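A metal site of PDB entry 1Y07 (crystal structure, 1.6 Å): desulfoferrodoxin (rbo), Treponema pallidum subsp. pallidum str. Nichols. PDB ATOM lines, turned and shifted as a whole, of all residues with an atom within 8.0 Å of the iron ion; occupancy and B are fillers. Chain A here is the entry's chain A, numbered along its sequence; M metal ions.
N of His 70 lies within hydrogen-bond range of O of Val 65, at 2.9 Å. The backbone carbonyl oxygen (O) of His 50 sits close to the side-chain carboxylate (OE2) of Glu 117 (2.6 Å). O of Ala 46 is in hydrogen-bond range of ND1 of His 50 (2.9 Å). The indole nitrogen of Trp 125 sits at hydrogen-bond distance from the backbone carbonyl oxygen of His 122, 2.8 Å away. The backbone NH (N) of Leu 121 lies close to the side-chain sulfur (SG) of Cys 119, at 3.4 Å. N of Cys 119 lies within hydrogen-bond range of OE1 of Glu 117.
Five residues have an atom within 4 Å of the iron ion: His 50, His 70, His 76, Cys 119 and His 122. The nearest printed residue that does not touch the iron ion is Leu 121 (4.9 Å).
The iron ion is bound by NE2 of His 70 (2.2 Å), NE2 of His 50 (2.2 Å), ND1 of His 122 (2.3 Å), SG of Cys 119 (2.3 Å) and NE2 of His 76 (2.4 Å).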
ATOM      1  N   VAL A  43       5.939 -18.732   8.182  1.00  0.00           N
ATOM      2  CA  VAL A  43       4.835 -17.867   8.575  1.00  0.00           C
ATOM      3  C   VAL A  43       3.781 -18.788   9.135  1.00  0.00           C
ATOM      4  O   VAL A  43       3.634 -19.907   8.693  1.00  0.00           O
ATOM      5  CB  VAL A  43       4.334 -16.985   7.379  1.00  0.00           C
ATOM      6  CG1 VAL A  43       2.979 -16.391   7.659  1.00  0.00           C
ATOM      7  CG2 VAL A  43       5.347 -15.876   7.105  1.00  0.00           C
ATOM      8  N   ALA A  45       0.796 -19.971   8.942  1.00  0.00           N
ATOM      9  CA  ALA A  45      -0.292 -20.015   7.953  1.00  0.00           C
ATOM     10  C   ALA A  45      -0.491 -21.460   7.509  1.00  0.00           C
ATOM     11  O   ALA A  45       0.378 -22.285   7.762  1.00  0.00           O
ATOM     12  CB  ALA A  45       0.019 -19.083   6.758  1.00  0.00           C
ATOM     13  N   ALA A  46      -1.607 -21.754   6.868  1.00  0.00           N
ATOM     14  CA  ALA A  46      -1.980 -23.131   6.501  1.00  0.00           C
ATOM     15  C   ALA A  46      -1.058 -23.688   5.428  1.00  0.00           C
ATOM     16  O   ALA A  46      -0.950 -23.129   4.325  1.00  0.00           O
ATOM     17  CB  ALA A  46      -3.409 -23.198   5.987  1.00  0.00           C
ATOM     18  N   LYS A  49      -2.624 -24.783   1.962  1.00  0.00           N
ATOM     19  CA  LYS A  49      -2.908 -23.781   0.997  1.00  0.00           C
ATOM     20  C   LYS A  49      -1.659 -23.097   0.492  1.00  0.00           C
ATOM     21  O   LYS A  49      -1.721 -22.332  -0.471  1.00  0.00           O
ATOM     22  CB  LYS A  49      -3.850 -22.737   1.637  1.00  0.00           C
ATOM     23  CG  LYS A  49      -5.267 -23.241   1.886  1.00  0.00           C
ATOM     24  CD  LYS A  49      -6.190 -22.072   2.310  1.00  0.00           C
ATOM     25  CE  LYS A  49      -7.712 -22.406   2.166  1.00  0.00           C
ATOM     26  NZ  LYS A  49      -8.365 -22.069   0.831  1.00  0.00           N
ATOM     27  N   HIS A  50      -0.491 -23.338   1.121  1.00  0.00           N
ATOM     28  CA  HIS A  50       0.715 -22.543   0.780  1.00  0.00           C
ATOM     29  C   HIS A  50       1.862 -23.375   0.187  1.00  0.00           C
ATOM     30  O   HIS A  50       2.644 -22.845  -0.591  1.00  0.00           O
ATOM     31  CB  HIS A  50       1.202 -21.757   2.048  1.00  0.00           C
ATOM     32  CG  HIS A  50       0.341 -20.575   2.334  1.00  0.00           C
ATOM     33  ND1 HIS A  50      -0.952 -20.714   2.805  1.00  0.00           N
ATOM     34  CD2 HIS A  50       0.497 -19.249   2.118  1.00  0.00           C
ATOM     35  CE1 HIS A  50      -1.546 -19.536   2.876  1.00  0.00           C
ATOM     36  NE2 HIS A  50      -0.727 -18.640   2.386  1.00  0.00           N
ATOM     37  N   VAL A  65      -0.717 -24.110  -6.070  1.00  0.00           N
ATOM     38  CA  VAL A  65      -0.600 -23.590  -4.732  1.00  0.00           C
ATOM     39  C   VAL A  65      -1.977 -23.609  -4.060  1.00  0.00           C
ATOM     40  O   VAL A  65      -2.817 -22.788  -4.437  1.00  0.00           O
ATOM     41  CB  VAL A  65      -0.074 -22.179  -4.701  1.00  0.00           C
ATOM     42  CG1 VAL A  65       0.222 -21.724  -3.258  1.00  0.00           C
ATOM     43  CG2 VAL A  65       1.211 -22.074  -5.481  1.00  0.00           C
ATOM     44  N   HIS A  70      -5.305 -22.006  -3.165  1.00  0.00           N
ATOM     45  CA  HIS A  70      -5.202 -20.760  -2.423  1.00  0.00           C
ATOM     46  C   HIS A  70      -6.041 -19.671  -3.063  1.00  0.00           C
ATOM     47  O   HIS A  70      -6.223 -19.683  -4.230  1.00  0.00           O
ATOM     48  CB  HIS A  70      -3.780 -20.301  -2.468  1.00  0.00           C
ATOM     49  CG  HIS A  70      -3.441 -19.162  -1.559  1.00  0.00           C
ATOM     50  ND1 HIS A  70      -3.047 -17.950  -2.035  1.00  0.00           N
ATOM     51  CD2 HIS A  70      -3.454 -19.050  -0.222  1.00  0.00           C
ATOM     52  CE1 HIS A  70      -2.697 -17.168  -1.023  1.00  0.00           C
ATOM     53  NE2 HIS A  70      -2.934 -17.829   0.084  1.00  0.00           N
ATOM     54  N   PRO A  71      -6.567 -18.750  -2.279  1.00  0.00           N
ATOM     55  CA  PRO A  71      -7.225 -17.571  -2.873  1.00  0.00           C
ATOM     56  C   PRO A  71      -6.413 -16.848  -3.908  1.00  0.00           C
ATOM     57  O   PRO A  71      -5.158 -16.786  -3.889  1.00  0.00           O
ATOM     58  CB  PRO A  71      -7.521 -16.685  -1.683  1.00  0.00           C
ATOM     59  CG  PRO A  71      -7.591 -17.650  -0.508  1.00  0.00           C
ATOM     60  CD  PRO A  71      -6.641 -18.760  -0.808  1.00  0.00           C
ATOM     61  N   GLU A  75      -6.897  -8.770  -2.560  1.00  0.00           N
ATOM     62  CA  GLU A  75      -6.331  -8.614  -1.225  1.00  0.00           C
ATOM     63  C   GLU A  75      -5.403  -9.777  -0.784  1.00  0.00           C
ATOM     64  O   GLU A  75      -4.562  -9.599   0.083  1.00  0.00           O
ATOM     65  CB  GLU A  75      -7.467  -8.457  -0.226  1.00  0.00           C
ATOM     66  CG  GLU A  75      -8.381  -9.659  -0.161  1.00  0.00           C
ATOM     67  CD  GLU A  75      -9.749  -9.493  -0.863  1.00  0.00           C
ATOM     68  OE1 GLU A  75      -9.790  -8.987  -2.059  1.00  0.00           O
ATOM     69  OE2 GLU A  75     -10.796  -9.936  -0.260  1.00  0.00           O
ATOM     70  N   HIS A  76      -5.538 -10.936  -1.425  1.00  0.00           N
ATOM     71  CA  HIS A  76      -4.878 -12.138  -0.917  1.00  0.00           C
ATOM     72  C   HIS A  76      -4.663 -13.071  -2.107  1.00  0.00           C
ATOM     73  O   HIS A  76      -5.599 -13.614  -2.636  1.00  0.00           O
ATOM     74  CB  HIS A  76      -5.763 -12.778   0.191  1.00  0.00           C
ATOM     75  CG  HIS A  76      -5.118 -13.958   0.820  1.00  0.00           C
ATOM     76  ND1 HIS A  76      -5.778 -15.129   0.991  1.00  0.00           N
ATOM     77  CD2 HIS A  76      -3.883 -14.133   1.347  1.00  0.00           C
ATOM     78  CE1 HIS A  76      -4.948 -16.031   1.496  1.00  0.00           C
ATOM     79  NE2 HIS A  76      -3.789 -15.447   1.696  1.00  0.00           N
ATOM     80  N   TYR A  77      -3.417 -13.186  -2.511  1.00  0.00           N
ATOM     81  CA  TYR A  77      -3.060 -13.822  -3.769  1.00  0.00           C
ATOM     82  C   TYR A  77      -1.641 -14.412  -3.745  1.00  0.00           C
ATOM     83  O   TYR A  77      -0.796 -13.992  -2.970  1.00  0.00           O
ATOM     84  CB  TYR A  77      -3.182 -12.783  -4.929  1.00  0.00           C
ATOM     85  CG  TYR A  77      -2.278 -11.586  -4.791  1.00  0.00           C
ATOM     86  CD1 TYR A  77      -0.939 -11.628  -5.162  1.00  0.00           C
ATOM     87  CD2 TYR A  77      -2.745 -10.404  -4.143  1.00  0.00           C
ATOM     88  CE1 TYR A  77      -0.130 -10.523  -4.983  1.00  0.00           C
ATOM     89  CE2 TYR A  77      -1.937  -9.327  -3.975  1.00  0.00           C
ATOM     90  CZ  TYR A  77      -0.639  -9.371  -4.392  1.00  0.00           C
ATOM     91  OH  TYR A  77       0.154  -8.231  -4.179  1.00  0.00           O
ATOM     92  N   ILE A  78      -1.434 -15.412  -4.607  1.00  0.00           N
ATOM     93  CA  ILE A  78      -0.100 -15.889  -4.962  1.00  0.00           C
ATOM     94  C   ILE A  78       0.426 -14.972  -6.092  1.00  0.00           C
ATOM     95  O   ILE A  78      -0.123 -14.916  -7.173  1.00  0.00           O
ATOM     96  CB  ILE A  78      -0.140 -17.372  -5.414  1.00  0.00           C
ATOM     97  CG1 ILE A  78      -0.817 -18.243  -4.321  1.00  0.00           C
ATOM     98  CG2 ILE A  78       1.256 -17.848  -5.735  1.00  0.00           C
ATOM     99  CD1 ILE A  78      -0.335 -17.996  -2.883  1.00  0.00           C
ATOM    100  N   GLU A 117       6.825 -20.387  -3.757  1.00  0.00           N
ATOM    101  CA  GLU A 117       5.738 -19.481  -4.129  1.00  0.00           C
ATOM    102  C   GLU A 117       5.692 -18.391  -3.057  1.00  0.00           C
ATOM    103  O   GLU A 117       6.030 -18.657  -1.911  1.00  0.00           O
ATOM    104  CB  GLU A 117       4.389 -20.238  -4.229  1.00  0.00           C
ATOM    105  CG  GLU A 117       3.837 -20.805  -2.940  1.00  0.00           C
ATOM    106  CD  GLU A 117       3.016 -19.862  -2.095  1.00  0.00           C
ATOM    107  OE1 GLU A 117       2.787 -18.731  -2.487  1.00  0.00           O
ATOM    108  OE2 GLU A 117       2.619 -20.282  -0.973  1.00  0.00           O
ATOM    109  N   PHE A 118       5.271 -17.181  -3.469  1.00  0.00           N
ATOM    110  CA  PHE A 118       5.076 -16.065  -2.538  1.00  0.00           C
ATOM    111  C   PHE A 118       3.588 -15.726  -2.499  1.00  0.00           C
ATOM    112  O   PHE A 118       2.992 -15.431  -3.532  1.00  0.00           O
ATOM    113  CB  PHE A 118       5.809 -14.872  -3.086  1.00  0.00           C
ATOM    114  CG  PHE A 118       5.669 -13.634  -2.248  1.00  0.00           C
ATOM    115  CD1 PHE A 118       6.107 -13.638  -0.953  1.00  0.00           C
ATOM    116  CD2 PHE A 118       5.112 -12.481  -2.772  1.00  0.00           C
ATOM    117  CE1 PHE A 118       5.971 -12.485  -0.227  1.00  0.00           C
ATOM    118  CE2 PHE A 118       5.008 -11.347  -2.020  1.00  0.00           C
ATOM    119  CZ  PHE A 118       5.408 -11.363  -0.791  1.00  0.00           C
ATOM    120  N   CYS A 119       3.010 -15.792  -1.315  1.00  0.00           N
ATOM    121  CA  CYS A 119       1.713 -15.214  -0.992  1.00  0.00           C
ATOM    122  C   CYS A 119       1.936 -13.794  -0.406  1.00  0.00           C
ATOM    123  O   CYS A 119       2.800 -13.630   0.447  1.00  0.00           O
ATOM    124  CB  CYS A 119       1.012 -16.102   0.035  1.00  0.00           C
ATOM    125  SG  CYS A 119      -0.433 -15.295   0.751  1.00  0.00           S
ATOM    126  N   ASN A 120       1.197 -12.811  -0.929  1.00  0.00           N
ATOM    127  CA  ASN A 120       1.365 -11.415  -0.504  1.00  0.00           C
ATOM    128  C   ASN A 120       1.199 -11.227   0.981  1.00  0.00           C
ATOM    129  O   ASN A 120       1.746 -10.249   1.524  1.00  0.00           O
ATOM    130  CB  ASN A 120       0.424 -10.484  -1.254  1.00  0.00           C
ATOM    131  CG  ASN A 120      -1.025 -10.613  -0.825  1.00  0.00           C
ATOM    132  OD1 ASN A 120      -1.616 -11.740  -0.841  1.00  0.00           O
ATOM    133  ND2 ASN A 120      -1.660  -9.479  -0.486  1.00  0.00           N
ATOM    134  N   LEU A 121       0.458 -12.097   1.649  1.00  0.00           N
ATOM    135  CA  LEU A 121       0.236 -12.009   3.091  1.00  0.00           C
ATOM    136  C   LEU A 121       1.050 -13.001   3.921  1.00  0.00           C
ATOM    137  O   LEU A 121       1.466 -12.714   5.050  1.00  0.00           O
ATOM    138  CB  LEU A 121      -1.251 -12.225   3.361  1.00  0.00           C
ATOM    139  CG  LEU A 121      -2.203 -11.174   2.763  1.00  0.00           C
ATOM    140  CD1 LEU A 121      -3.632 -11.345   3.255  1.00  0.00           C
ATOM    141  CD2 LEU A 121      -1.746  -9.756   3.077  1.00  0.00           C
ATOM    142  N   HIS A 122       1.312 -14.166   3.349  1.00  0.00           N
ATOM    143  CA  HIS A 122       1.845 -15.322   4.094  1.00  0.00           C
ATOM    144  C   HIS A 122       3.246 -15.754   3.727  1.00  0.00           C
ATOM    145  O   HIS A 122       3.741 -16.772   4.231  1.00  0.00           O
ATOM    146  CB  HIS A 122       0.823 -16.436   4.005  1.00  0.00           C
ATOM    147  CG  HIS A 122      -0.480 -16.068   4.589  1.00  0.00           C
ATOM    148  ND1 HIS A 122      -1.667 -16.307   3.969  1.00  0.00           N
ATOM    149  CD2 HIS A 122      -0.767 -15.423   5.748  1.00  0.00           C
ATOM    150  CE1 HIS A 122      -2.657 -15.855   4.724  1.00  0.00           C
ATOM    151  NE2 HIS A 122      -2.140 -15.312   5.814  1.00  0.00           N
ATOM    152  N   GLY A 123       3.938 -14.923   2.961  1.00  0.00           N
ATOM    153  CA  GLY A 123       5.353 -15.119   2.694  1.00  0.00           C
ATOM    154  C   GLY A 123       5.674 -16.188   1.634  1.00  0.00           C
ATOM    155  O   GLY A 123       4.824 -16.622   0.851  1.00  0.00           O
ATOM    156  N   TRP A 125       7.032 -19.955   0.499  1.00  0.00           N
ATOM    157  CA  TRP A 125       6.946 -21.348   0.867  1.00  0.00           C
ATOM    158  C   TRP A 125       7.596 -22.198  -0.200  1.00  0.00           C
ATOM    159  O   TRP A 125       7.453 -21.898  -1.396  1.00  0.00           O
ATOM    160  CB  TRP A 125       5.486 -21.776   0.994  1.00  0.00           C
ATOM    161  CG  TRP A 125       4.792 -21.052   2.107  1.00  0.00           C
ATOM    162  CD1 TRP A 125       4.342 -19.778   2.085  1.00  0.00           C
ATOM    163  CD2 TRP A 125       4.500 -21.569   3.388  1.00  0.00           C
ATOM    164  NE1 TRP A 125       3.820 -19.443   3.306  1.00  0.00           N
ATOM    165  CE2 TRP A 125       3.906 -20.524   4.127  1.00  0.00           C
ATOM    166  CE3 TRP A 125       4.742 -22.799   4.015  1.00  0.00           C
ATOM    167  CZ2 TRP A 125       3.441 -20.701   5.427  1.00  0.00           C
ATOM    168  CZ3 TRP A 125       4.306 -22.957   5.323  1.00  0.00           C
ATOM    169  CH2 TRP A 125       3.672 -21.913   6.017  1.00  0.00           C
HETATM  170 FE    FE M   1      -1.880 -16.834   1.737  1.00  0.00          FE
